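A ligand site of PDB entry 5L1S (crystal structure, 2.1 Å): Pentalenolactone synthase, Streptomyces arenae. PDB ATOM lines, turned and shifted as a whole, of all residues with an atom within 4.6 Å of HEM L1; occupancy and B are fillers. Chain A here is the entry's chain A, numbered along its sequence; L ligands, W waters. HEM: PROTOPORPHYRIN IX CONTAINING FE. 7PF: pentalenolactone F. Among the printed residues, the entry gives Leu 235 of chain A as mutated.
SG of Cys 350 is bound to FE of HEM L1 (2.4 Å).
The guanidinium group (NH2) of Arg 291 is in salt-bridge range of an oxygen (O1A) of HEM L1 (2.7 Å).
The guanidinium group (NH1) of Arg 100 lies within salt-bridge range of an oxygen (O1D) of HEM L1, 2.7 Å away.
An oxygen (O1D) of HEM L1 sits at hydrogen-bond distance from a ring nitrogen (NE2) of His 96 (2.7 Å).
The guanidinium group of Arg 348 is in salt-bridge range of an oxygen (O2D) of HEM L1, at 2.8 Å.
The guanidinium group of Arg 243 lies within salt-bridge range of an oxygen (O4) of 7PF L2, at 2.8 Å.
N of Gly 352 sits close to SG of Cys 350 (3.5 Å).
The backbone carbonyl oxygen (O) of Phe 343 is in hydrogen-bond range of the backbone NH (N) of Cys 350.
The backbone carbonyl oxygen (O) of Ala 347 lies close to the guanidinium group (NE) of Arg 100, at 3.2 Å.
The backbone carbonyl oxygen of His 349 sits at hydrogen-bond distance from the guanidinium group of Arg 100, 2.9 Å away.
The guanidinium group (NH1) of Arg 348 sits close to a ring nitrogen (NE2) of His 96.
The backbone carbonyl oxygen of Met 84 lies within hydrogen-bond range of the guanidinium group of Arg 348 (2.9 Å).
The backbone carbonyl oxygen (O) of Thr 239 lies within hydrogen-bond range of the guanidinium group (NH1) of Arg 243, at 3.0 Å.
Residues that only touch HEM L1: Thr 239, Ala 342, Arg 243, Gly 236, Gly 352, Met 84, Phe 343, Thr 240, Gly 344, Ile 289, Leu 235, Phe 107, Ile 351, Ala 356 and Leu 155.
Hydrophobic or aromatic side chains that line HEM L1: Met 84, His 96, Phe 107, Leu 155, Leu 235, Ile 289, Phe 343 and Ala 356.
20 residues have an atom within 4 Å of HEM L1: Met 84, His 96, Arg 100, Phe 107, Leu 155, Leu 235, Gly 236, Thr 239, Thr 240, Arg 243, Ile 289, Arg 291, Ala 342, Phe 343, Gly 344, Arg 348, Cys 350, Ile 351, Gly 352 and Ala 356.
The nearest printed residue that does not touch HEM L1 is Ala 347 (4.1 Å).
Water W3 bridges an oxygen (O1A) of HEM L1 and the backbone carbonyl oxygen of Arg 348.
Water W1 lies within hydrogen-bond range of O2A of HEM L1 (2.8 Å) and O2 of 7PF L2 (3.0 Å).
Water W4 lies within hydrogen-bond range of O of Leu 235 and OG1 of Thr 239.
Water W2 lies within hydrogen-bond range of OG1 of Thr 239 (2.7 Å), OG1 of Thr 240 (2.7 Å), O of Leu 235 (3.1 Å) and O of Gly 236 (3.5 Å).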
ATOM      1  N   LEU A  63      31.204  -6.877   4.279  1.00  0.00           N
ATOM      2  CA  LEU A  63      31.075  -5.466   4.625  1.00  0.00           C
ATOM      3  C   LEU A  63      32.436  -4.796   4.734  1.00  0.00           C
ATOM      4  O   LEU A  63      32.606  -3.652   4.287  1.00  0.00           O
ATOM      5  CB  LEU A  63      30.302  -5.321   5.946  1.00  0.00           C
ATOM      6  CG  LEU A  63      30.012  -3.892   6.417  1.00  0.00           C
ATOM      7  CD1 LEU A  63      28.992  -3.183   5.481  1.00  0.00           C
ATOM      8  CD2 LEU A  63      29.524  -3.872   7.868  1.00  0.00           C
ATOM      9  N   MET A  84      28.749  -2.470  13.201  1.00  0.00           N
ATOM     10  CA  MET A  84      28.472  -3.770  12.584  1.00  0.00           C
ATOM     11  C   MET A  84      29.704  -4.663  12.539  1.00  0.00           C
ATOM     12  O   MET A  84      29.696  -5.674  11.806  1.00  0.00           O
ATOM     13  CB  MET A  84      27.914  -3.549  11.171  1.00  0.00           C
ATOM     14  CG  MET A  84      26.508  -2.922  11.183  1.00  0.00           C
ATOM     15  SD  MET A  84      25.970  -2.291   9.580  1.00  0.00           S
ATOM     16  CE  MET A  84      25.667  -3.821   8.676  1.00  0.00           C
ATOM     17  N   HIS A  96      32.158 -10.426  13.905  1.00  0.00           N
ATOM     18  CA  HIS A  96      30.790 -10.417  13.398  1.00  0.00           C
ATOM     19  C   HIS A  96      30.027 -11.645  13.872  1.00  0.00           C
ATOM     20  O   HIS A  96      28.852 -11.546  14.252  1.00  0.00           O
ATOM     21  CB  HIS A  96      30.740 -10.335  11.874  1.00  0.00           C
ATOM     22  CG  HIS A  96      29.352 -10.320  11.338  1.00  0.00           C
ATOM     23  ND1 HIS A  96      28.850 -11.321  10.530  1.00  0.00           N
ATOM     24  CD2 HIS A  96      28.332  -9.446  11.533  1.00  0.00           C
ATOM     25  CE1 HIS A  96      27.585 -11.050  10.235  1.00  0.00           C
ATOM     26  NE2 HIS A  96      27.251  -9.911  10.828  1.00  0.00           N
ATOM     27  N   MET A  99      28.967 -10.997  17.390  1.00  0.00           N
ATOM     28  CA  MET A  99      27.904 -10.007  17.444  1.00  0.00           C
ATOM     29  C   MET A  99      26.547 -10.644  17.222  1.00  0.00           C
ATOM     30  O   MET A  99      25.613 -10.431  18.011  1.00  0.00           O
ATOM     31  CB  MET A  99      28.166  -8.909  16.414  1.00  0.00           C
ATOM     32  CG  MET A  99      27.073  -7.877  16.366  1.00  0.00           C
ATOM     33  SD  MET A  99      27.327  -6.688  15.020  1.00  0.00           S
ATOM     34  CE  MET A  99      25.930  -5.573  15.338  1.00  0.00           C
ATOM     35  N   ARG A 100      26.399 -11.418  16.144  1.00  0.00           N
ATOM     36  CA  ARG A 100      25.129 -12.082  15.870  1.00  0.00           C
ATOM     37  C   ARG A 100      24.791 -13.113  16.953  1.00  0.00           C
ATOM     38  O   ARG A 100      23.643 -13.219  17.380  1.00  0.00           O
ATOM     39  CB  ARG A 100      25.168 -12.731  14.492  1.00  0.00           C
ATOM     40  CG  ARG A 100      25.110 -11.681  13.356  1.00  0.00           C
ATOM     41  CD  ARG A 100      24.872 -12.353  12.033  1.00  0.00           C
ATOM     42  NE  ARG A 100      23.480 -12.808  11.838  1.00  0.00           N
ATOM     43  CZ  ARG A 100      22.473 -12.036  11.429  1.00  0.00           C
ATOM     44  NH1 ARG A 100      22.644 -10.738  11.149  1.00  0.00           N
ATOM     45  NH2 ARG A 100      21.276 -12.582  11.258  1.00  0.00           N
ATOM     46  N   LEU A 103      23.393 -11.126  19.894  1.00  0.00           N
ATOM     47  CA  LEU A 103      22.175 -10.333  19.729  1.00  0.00           C
ATOM     48  C   LEU A 103      20.940 -11.177  19.391  1.00  0.00           C
ATOM     49  O   LEU A 103      19.826 -10.834  19.808  1.00  0.00           O
ATOM     50  CB  LEU A 103      22.385  -9.264  18.640  1.00  0.00           C
ATOM     51  CG  LEU A 103      23.293  -8.075  19.003  1.00  0.00           C
ATOM     52  CD1 LEU A 103      23.573  -7.184  17.786  1.00  0.00           C
ATOM     53  CD2 LEU A 103      22.695  -7.247  20.139  1.00  0.00           C
ATOM     54  N   PHE A 107      16.199 -11.438  21.031  1.00  0.00           N
ATOM     55  CA  PHE A 107      14.900 -11.253  20.398  1.00  0.00           C
ATOM     56  C   PHE A 107      14.119 -12.566  20.404  1.00  0.00           C
ATOM     57  O   PHE A 107      13.659 -13.041  19.367  1.00  0.00           O
ATOM     58  CB  PHE A 107      15.094 -10.693  18.979  1.00  0.00           C
ATOM     59  CG  PHE A 107      15.742  -9.314  18.955  1.00  0.00           C
ATOM     60  CD1 PHE A 107      17.114  -9.184  18.977  1.00  0.00           C
ATOM     61  CD2 PHE A 107      14.963  -8.162  18.945  1.00  0.00           C
ATOM     62  CE1 PHE A 107      17.704  -7.928  18.989  1.00  0.00           C
ATOM     63  CE2 PHE A 107      15.550  -6.910  18.949  1.00  0.00           C
ATOM     64  CZ  PHE A 107      16.926  -6.789  18.972  1.00  0.00           C
ATOM     65  N   LEU A 155      13.337  -2.360  25.020  1.00  0.00           N
ATOM     66  CA  LEU A 155      14.457  -3.272  24.844  1.00  0.00           C
ATOM     67  C   LEU A 155      15.600  -2.920  25.802  1.00  0.00           C
ATOM     68  O   LEU A 155      16.246  -3.816  26.352  1.00  0.00           O
ATOM     69  CB  LEU A 155      14.979  -3.226  23.406  1.00  0.00           C
ATOM     70  CG  LEU A 155      14.128  -3.845  22.294  1.00  0.00           C
ATOM     71  CD1 LEU A 155      14.746  -3.525  20.947  1.00  0.00           C
ATOM     72  CD2 LEU A 155      14.035  -5.355  22.482  1.00  0.00           C
ATOM     73  N   LEU A 235      20.514   1.380  15.388  1.00  0.00           N
ATOM     74  CA  LEU A 235      19.849   0.674  14.290  1.00  0.00           C
ATOM     75  C   LEU A 235      18.405   0.296  14.623  1.00  0.00           C
ATOM     76  O   LEU A 235      17.654  -0.078  13.709  1.00  0.00           O
ATOM     77  CB  LEU A 235      20.631  -0.591  13.909  1.00  0.00           C
ATOM     78  CG  LEU A 235      22.167  -0.423  13.800  1.00  0.00           C
ATOM     79  CD1 LEU A 235      22.864  -1.700  13.356  1.00  0.00           C
ATOM     80  CD2 LEU A 235      22.571   0.768  12.911  1.00  0.00           C
ATOM     81  N   GLY A 236      18.006   0.383  15.881  1.00  0.00           N
ATOM     82  CA  GLY A 236      16.761  -0.229  16.302  1.00  0.00           C
ATOM     83  C   GLY A 236      15.507   0.618  16.248  1.00  0.00           C
ATOM     84  O   GLY A 236      14.436   0.090  16.561  1.00  0.00           O
ATOM     85  N   THR A 239      15.089   3.357  11.183  1.00  0.00           N
ATOM     86  CA  THR A 239      14.602   2.762   9.939  1.00  0.00           C
ATOM     87  C   THR A 239      13.146   2.323  10.042  1.00  0.00           C
ATOM     88  O   THR A 239      12.423   2.355   9.045  1.00  0.00           O
ATOM     89  CB  THR A 239      15.472   1.566   9.521  1.00  0.00           C
ATOM     90  OG1 THR A 239      15.459   0.571  10.555  1.00  0.00           O
ATOM     91  CG2 THR A 239      16.939   2.001   9.235  1.00  0.00           C
ATOM     92  N   THR A 240      12.708   1.894  11.224  1.00  0.00           N
ATOM     93  CA  THR A 240      11.300   1.565  11.446  1.00  0.00           C
ATOM     94  C   THR A 240      10.429   2.815  11.324  1.00  0.00           C
ATOM     95  O   THR A 240       9.370   2.778  10.695  1.00  0.00           O
ATOM     96  CB  THR A 240      11.113   0.907  12.822  1.00  0.00           C
ATOM     97  OG1 THR A 240      12.024  -0.189  12.936  1.00  0.00           O
ATOM     98  CG2 THR A 240       9.700   0.378  12.983  1.00  0.00           C
ATOM     99  N   ARG A 243       9.864   3.453   7.778  1.00  0.00           N
ATOM    100  CA  ARG A 243       8.895   2.566   7.134  1.00  0.00           C
ATOM    101  C   ARG A 243       7.456   2.865   7.518  1.00  0.00           C
ATOM    102  O   ARG A 243       6.533   2.606   6.727  1.00  0.00           O
ATOM    103  CB  ARG A 243       9.217   1.090   7.412  1.00  0.00           C
ATOM    104  CG  ARG A 243      10.613   0.656   6.884  1.00  0.00           C
ATOM    105  CD  ARG A 243      10.864   1.319   5.535  1.00  0.00           C
ATOM    106  NE  ARG A 243      12.120   0.977   4.873  1.00  0.00           N
ATOM    107  CZ  ARG A 243      13.310   1.455   5.210  1.00  0.00           C
ATOM    108  NH1 ARG A 243      13.464   2.281   6.249  1.00  0.00           N
ATOM    109  NH2 ARG A 243      14.387   1.095   4.508  1.00  0.00           N
ATOM    110  N   LEU A 276       7.269  -2.870   2.888  1.00  0.00           N
ATOM    111  CA  LEU A 276       8.718  -3.084   2.939  1.00  0.00           C
ATOM    112  C   LEU A 276       9.299  -3.218   1.534  1.00  0.00           C
ATOM    113  O   LEU A 276      10.366  -2.676   1.240  1.00  0.00           O
ATOM    114  CB  LEU A 276       9.030  -4.333   3.761  1.00  0.00           C
ATOM    115  CG  LEU A 276       8.592  -4.318   5.228  1.00  0.00           C
ATOM    116  CD1 LEU A 276       8.657  -5.704   5.894  1.00  0.00           C
ATOM    117  CD2 LEU A 276       9.462  -3.325   5.952  1.00  0.00           C
ATOM    118  N   ILE A 289      22.897  -1.954  -0.326  1.00  0.00           N
ATOM    119  CA  ILE A 289      23.703  -2.627   0.681  1.00  0.00           C
ATOM    120  C   ILE A 289      25.138  -2.650   0.169  1.00  0.00           C
ATOM    121  O   ILE A 289      25.406  -3.256  -0.881  1.00  0.00           O
ATOM    122  CB  ILE A 289      23.210  -4.050   0.965  1.00  0.00           C
ATOM    123  CG1 ILE A 289      21.849  -4.017   1.701  1.00  0.00           C
ATOM    124  CG2 ILE A 289      24.299  -4.820   1.742  1.00  0.00           C
ATOM    125  CD1 ILE A 289      21.294  -5.437   2.084  1.00  0.00           C
ATOM    126  N   ARG A 291      29.166  -3.523  -0.178  1.00  0.00           N
ATOM    127  CA  ARG A 291      30.056  -4.643   0.066  1.00  0.00           C
ATOM    128  C   ARG A 291      31.398  -4.393  -0.638  1.00  0.00           C
ATOM    129  O   ARG A 291      31.512  -3.550  -1.517  1.00  0.00           O
ATOM    130  CB  ARG A 291      29.469  -5.973  -0.453  1.00  0.00           C
ATOM    131  CG  ARG A 291      28.217  -6.469   0.277  1.00  0.00           C
ATOM    132  CD  ARG A 291      28.527  -6.862   1.730  1.00  0.00           C
ATOM    133  NE  ARG A 291      27.386  -7.479   2.393  1.00  0.00           N
ATOM    134  CZ  ARG A 291      26.597  -6.882   3.294  1.00  0.00           C
ATOM    135  NH1 ARG A 291      26.829  -5.625   3.676  1.00  0.00           N
ATOM    136  NH2 ARG A 291      25.586  -7.567   3.832  1.00  0.00           N
ATOM    137  N   ILE A 314      18.940  -3.512  -3.162  1.00  0.00           N
ATOM    138  CA  ILE A 314      17.784  -4.245  -2.666  1.00  0.00           C
ATOM    139  C   ILE A 314      16.485  -3.531  -3.044  1.00  0.00           C
ATOM    140  O   ILE A 314      15.472  -4.180  -3.312  1.00  0.00           O
ATOM    141  CB  ILE A 314      17.895  -4.442  -1.128  1.00  0.00           C
ATOM    142  CG1 ILE A 314      18.022  -3.096  -0.392  1.00  0.00           C
ATOM    143  CG2 ILE A 314      19.076  -5.392  -0.776  1.00  0.00           C
ATOM    144  CD1 ILE A 314      18.033  -3.218   1.146  1.00  0.00           C
ATOM    145  N   ALA A 342      14.175  -6.316   1.632  1.00  0.00           N
ATOM    146  CA  ALA A 342      14.301  -5.076   2.406  1.00  0.00           C
ATOM    147  C   ALA A 342      15.018  -5.260   3.740  1.00  0.00           C
ATOM    148  O   ALA A 342      15.527  -4.269   4.298  1.00  0.00           O
ATOM    149  CB  ALA A 342      12.933  -4.442   2.660  1.00  0.00           C
ATOM    150  N   PHE A 343      15.042  -6.467   4.282  1.00  0.00           N
ATOM    151  CA  PHE A 343      15.842  -6.770   5.466  1.00  0.00           C
ATOM    152  C   PHE A 343      17.182  -7.397   5.113  1.00  0.00           C
ATOM    153  O   PHE A 343      17.882  -7.924   5.994  1.00  0.00           O
ATOM    154  CB  PHE A 343      15.060  -7.702   6.409  1.00  0.00           C
ATOM    155  CG  PHE A 343      13.848  -7.065   7.068  1.00  0.00           C
ATOM    156  CD1 PHE A 343      13.978  -5.944   7.861  1.00  0.00           C
ATOM    157  CD2 PHE A 343      12.586  -7.654   6.947  1.00  0.00           C
ATOM    158  CE1 PHE A 343      12.850  -5.373   8.500  1.00  0.00           C
ATOM    159  CE2 PHE A 343      11.463  -7.117   7.576  1.00  0.00           C
ATOM    160  CZ  PHE A 343      11.596  -5.964   8.352  1.00  0.00           C
ATOM    161  N   GLY A 344      17.549  -7.383   3.823  1.00  0.00           N
ATOM    162  CA  GLY A 344      18.741  -8.078   3.392  1.00  0.00           C
ATOM    163  C   GLY A 344      18.539  -9.587   3.329  1.00  0.00           C
ATOM    164  O   GLY A 344      17.418 -10.096   3.201  1.00  0.00           O
ATOM    165  N   ALA A 347      24.398 -13.573   5.518  1.00  0.00           N
ATOM    166  CA  ALA A 347      25.159 -13.468   6.769  1.00  0.00           C
ATOM    167  C   ALA A 347      24.698 -12.302   7.646  1.00  0.00           C
ATOM    168  O   ALA A 347      24.712 -12.428   8.872  1.00  0.00           O
ATOM    169  CB  ALA A 347      26.652 -13.335   6.456  1.00  0.00           C
ATOM    170  N   ARG A 348      24.290 -11.185   7.049  1.00  0.00           N
ATOM    171  CA  ARG A 348      23.936  -9.984   7.801  1.00  0.00           C
ATOM    172  C   ARG A 348      22.439  -9.692   7.796  1.00  0.00           C
ATOM    173  O   ARG A 348      22.026  -8.563   8.082  1.00  0.00           O
ATOM    174  CB  ARG A 348      24.750  -8.798   7.287  1.00  0.00           C
ATOM    175  CG  ARG A 348      26.242  -8.913   7.619  1.00  0.00           C
ATOM    176  CD  ARG A 348      27.049  -7.660   7.209  1.00  0.00           C
ATOM    177  NE  ARG A 348      28.439  -7.715   7.667  1.00  0.00           N
ATOM    178  CZ  ARG A 348      28.855  -7.294   8.858  1.00  0.00           C
ATOM    179  NH1 ARG A 348      27.981  -6.794   9.725  1.00  0.00           N
ATOM    180  NH2 ARG A 348      30.130  -7.379   9.193  1.00  0.00           N
ATOM    181  N   HIS A 349      21.618 -10.697   7.498  1.00  0.00           N
ATOM    182  CA  HIS A 349      20.164 -10.578   7.542  1.00  0.00           C
ATOM    183  C   HIS A 349      19.711  -9.880   8.839  1.00  0.00           C
ATOM    184  O   HIS A 349      20.043 -10.333   9.939  1.00  0.00           O
ATOM    185  CB  HIS A 349      19.575 -11.998   7.462  1.00  0.00           C
ATOM    186  CG  HIS A 349      18.160 -12.057   6.960  1.00  0.00           C
ATOM    187  ND1 HIS A 349      17.479 -13.255   6.855  1.00  0.00           N
ATOM    188  CD2 HIS A 349      17.311 -11.096   6.534  1.00  0.00           C
ATOM    189  CE1 HIS A 349      16.262 -13.021   6.400  1.00  0.00           C
ATOM    190  NE2 HIS A 349      16.130 -11.721   6.188  1.00  0.00           N
ATOM    191  N   CYS A 350      19.008  -8.735   8.689  1.00  0.00           N
ATOM    192  CA  CYS A 350      18.392  -8.001   9.805  1.00  0.00           C
ATOM    193  C   CYS A 350      18.057  -8.821  11.051  1.00  0.00           C
ATOM    194  O   CYS A 350      17.210  -9.710  11.010  1.00  0.00           O
ATOM    195  CB  CYS A 350      17.111  -7.309   9.345  1.00  0.00           C
ATOM    196  SG  CYS A 350      16.474  -6.208  10.611  1.00  0.00           S
ATOM    197  N   ILE A 351      18.672  -8.454  12.175  1.00  0.00           N
ATOM    198  CA  ILE A 351      18.406  -9.142  13.447  1.00  0.00           C
ATOM    199  C   ILE A 351      17.062  -8.713  14.037  1.00  0.00           C
ATOM    200  O   ILE A 351      16.385  -9.525  14.683  1.00  0.00           O
ATOM    201  CB  ILE A 351      19.564  -8.883  14.417  1.00  0.00           C
ATOM    202  CG1 ILE A 351      20.850  -9.569  13.925  1.00  0.00           C
ATOM    203  CG2 ILE A 351      19.229  -9.375  15.845  1.00  0.00           C
ATOM    204  CD1 ILE A 351      22.059  -9.301  14.784  1.00  0.00           C
ATOM    205  N   GLY A 352      16.630  -7.471  13.824  1.00  0.00           N
ATOM    206  CA  GLY A 352      15.371  -7.017  14.387  1.00  0.00           C
ATOM    207  C   GLY A 352      14.144  -7.225  13.533  1.00  0.00           C
ATOM    208  O   GLY A 352      13.065  -6.700  13.872  1.00  0.00           O
ATOM    209  N   LEU A 355      10.779  -8.257  15.051  1.00  0.00           N
ATOM    210  CA  LEU A 355      10.260  -7.160  15.856  1.00  0.00           C
ATOM    211  C   LEU A 355       9.756  -6.020  14.981  1.00  0.00           C
ATOM    212  O   LEU A 355       8.692  -5.438  15.239  1.00  0.00           O
ATOM    213  CB  LEU A 355      11.338  -6.675  16.842  1.00  0.00           C
ATOM    214  CG  LEU A 355      10.958  -5.499  17.737  1.00  0.00           C
ATOM    215  CD1 LEU A 355       9.716  -5.820  18.560  1.00  0.00           C
ATOM    216  CD2 LEU A 355      12.117  -5.106  18.644  1.00  0.00           C
ATOM    217  N   ALA A 356      10.513  -5.661  13.935  1.00  0.00           N
ATOM    218  CA  ALA A 356      10.076  -4.585  13.035  1.00  0.00           C
ATOM    219  C   ALA A 356       8.746  -4.932  12.390  1.00  0.00           C
ATOM    220  O   ALA A 356       7.864  -4.068  12.251  1.00  0.00           O
ATOM    221  CB  ALA A 356      11.127  -4.317  11.955  1.00  0.00           C
ATOM    222  N   GLU A 359       5.875  -4.316  14.907  1.00  0.00           N
ATOM    223  CA  GLU A 359       5.536  -2.891  14.984  1.00  0.00           C
ATOM    224  C   GLU A 359       4.698  -2.447  13.800  1.00  0.00           C
ATOM    225  O   GLU A 359       3.650  -1.821  13.969  1.00  0.00           O
ATOM    226  CB  GLU A 359       6.818  -2.043  15.047  1.00  0.00           C
ATOM    227  CG  GLU A 359       7.629  -2.217  16.320  1.00  0.00           C
ATOM    228  CD  GLU A 359       8.809  -1.261  16.379  1.00  0.00           C
ATOM    229  OE1 GLU A 359       8.613  -0.024  16.226  1.00  0.00           O
ATOM    230  OE2 GLU A 359       9.940  -1.758  16.530  1.00  0.00           O
ATOM    231  N   LEU A 360       5.157  -2.747  12.578  1.00  0.00           N
ATOM    232  CA  LEU A 360       4.445  -2.262  11.400  1.00  0.00           C
ATOM    233  C   LEU A 360       3.075  -2.907  11.271  1.00  0.00           C
ATOM    234  O   LEU A 360       2.087  -2.239  10.914  1.00  0.00           O
ATOM    235  CB  LEU A 360       5.293  -2.460  10.129  1.00  0.00           C
ATOM    236  CG  LEU A 360       6.650  -1.743  10.062  1.00  0.00           C
ATOM    237  CD1 LEU A 360       7.556  -2.278   8.933  1.00  0.00           C
ATOM    238  CD2 LEU A 360       6.513  -0.208   9.934  1.00  0.00           C
HETATM  239  CHA HEM L   1      20.805  -5.248   9.552  1.00  0.00           C
HETATM  240  CHB HEM L   1      16.927  -3.289   7.369  1.00  0.00           C
HETATM  241  CHC HEM L   1      14.852  -2.655  11.713  1.00  0.00           C
HETATM  242  CHD HEM L   1      18.800  -4.392  13.915  1.00  0.00           C
HETATM  243  C1A HEM L   1      19.930  -4.833   8.566  1.00  0.00           C
HETATM  244  C2A HEM L   1      20.131  -4.945   7.136  1.00  0.00           C
HETATM  245  C3A HEM L   1      19.052  -4.394   6.529  1.00  0.00           C
HETATM  246  C4A HEM L   1      18.136  -3.931   7.564  1.00  0.00           C
HETATM  247  CMA HEM L   1      18.787  -4.245   5.013  1.00  0.00           C
HETATM  248  CAA HEM L   1      21.361  -5.602   6.454  1.00  0.00           C
HETATM  249  CBA HEM L   1      22.526  -4.623   6.305  1.00  0.00           C
HETATM  250  CGA HEM L   1      23.646  -5.261   5.497  1.00  0.00           C
HETATM  251  O1A HEM L   1      23.469  -6.406   4.990  1.00  0.00           O
HETATM  252  O2A HEM L   1      24.720  -4.619   5.369  1.00  0.00           O
HETATM  253  C1B HEM L   1      16.015  -2.920   8.338  1.00  0.00           C
HETATM  254  C2B HEM L   1      14.706  -2.331   8.131  1.00  0.00           C
HETATM  255  C3B HEM L   1      14.150  -2.157   9.362  1.00  0.00           C
HETATM  256  C4B HEM L   1      15.081  -2.658  10.350  1.00  0.00           C
HETATM  257  CMB HEM L   1      14.081  -1.951   6.758  1.00  0.00           C
HETATM  258  CAB HEM L   1      12.767  -1.589   9.750  1.00  0.00           C
HETATM  259  CBB HEM L   1      11.665  -1.798   9.017  1.00  0.00           C
HETATM  260  C1C HEM L   1      15.699  -3.104  12.715  1.00  0.00           C
HETATM  261  C2C HEM L   1      15.391  -3.195  14.134  1.00  0.00           C
HETATM  262  C3C HEM L   1      16.497  -3.689  14.738  1.00  0.00           C
HETATM  263  C4C HEM L   1      17.522  -3.897  13.725  1.00  0.00           C
HETATM  264  CMC HEM L   1      14.015  -2.790  14.739  1.00  0.00           C
HETATM  265  CAC HEM L   1      16.754  -3.981  16.241  1.00  0.00           C
HETATM  266  CBC HEM L   1      15.987  -3.544  17.243  1.00  0.00           C
HETATM  267  C1D HEM L   1      19.702  -4.715  12.917  1.00  0.00           C
HETATM  268  C2D HEM L   1      21.082  -5.108  13.131  1.00  0.00           C
HETATM  269  C3D HEM L   1      21.636  -5.334  11.926  1.00  0.00           C
HETATM  270  C4D HEM L   1      20.632  -5.092  10.913  1.00  0.00           C
HETATM  271  CMD HEM L   1      21.747  -5.225  14.518  1.00  0.00           C
HETATM  272  CAD HEM L   1      23.075  -5.782  11.635  1.00  0.00           C
HETATM  273  CBD HEM L   1      23.052  -7.282  11.330  1.00  0.00           C
HETATM  274  CGD HEM L   1      24.440  -7.768  10.937  1.00  0.00           C
HETATM  275  O1D HEM L   1      24.710  -9.000  11.053  1.00  0.00           O
HETATM  276  O2D HEM L   1      25.285  -6.916  10.542  1.00  0.00           O
HETATM  277  NA  HEM L   1      18.710  -4.210   8.793  1.00  0.00           N
HETATM  278  NB  HEM L   1      16.205  -3.097   9.699  1.00  0.00           N
HETATM  279  NC  HEM L   1      16.995  -3.545  12.512  1.00  0.00           N
HETATM  280  ND  HEM L   1      19.482  -4.723  11.562  1.00  0.00           N
HETATM  281 FE   HEM L   1      17.730  -4.121  10.656  1.00  0.00          FE
HETATM  282  C1  7PF L   2      20.255  -1.469   7.955  1.00  0.00           C
HETATM  283  C2  7PF L   2      21.326  -0.603   8.634  1.00  0.00           C
HETATM  284  C15 7PF L   2      22.167  -1.457   9.577  1.00  0.00           C
HETATM  285  C14 7PF L   2      20.719   0.568   9.457  1.00  0.00           C
HETATM  286  C7  7PF L   2      18.932  -0.274   6.141  1.00  0.00           C
HETATM  287  C12 7PF L   2      20.968   2.254   5.103  1.00  0.00           C
HETATM  288  C10 7PF L   2      21.276  -0.799   3.718  1.00  0.00           C
HETATM  289  C3  7PF L   2      22.209  -0.173   7.436  1.00  0.00           C
HETATM  290  C13 7PF L   2      18.103   1.960   5.791  1.00  0.00           C
HETATM  291  C11 7PF L   2      22.906   0.855   4.667  1.00  0.00           C
HETATM  292  C6  7PF L   2      19.103   1.070   6.103  1.00  0.00           C
HETATM  293  C8  7PF L   2      20.138  -1.002   6.461  1.00  0.00           C
HETATM  294  C5  7PF L   2      20.466   1.402   6.322  1.00  0.00           C
HETATM  295  C9  7PF L   2      21.971  -0.160   4.905  1.00  0.00           C
HETATM  296  C4  7PF L   2      21.224   0.053   6.266  1.00  0.00           C
HETATM  297  O4  7PF L   2      16.960   1.562   5.454  1.00  0.00           O
HETATM  298  O2  7PF L   2      24.090   0.603   4.391  1.00  0.00           O
HETATM  299  O5  7PF L   2      18.253   3.199   5.837  1.00  0.00           O
HETATM  300  O3  7PF L   2      22.437   2.132   4.826  1.00  0.00           O
HETATM  301  O1  7PF L   2      22.302  -1.498   4.491  1.00  0.00           O
HETATM  302  O   HOH W   1      25.322  -1.897   5.373  1.00  0.00           O
HETATM  303  O   HOH W   2      14.662   0.498  13.127  1.00  0.00           O
HETATM  304  O   HOH W   3      21.910  -8.634   4.600  1.00  0.00           O
HETATM  305  O   HOH W   4      17.915  -0.802  11.112  1.00  0.00           O
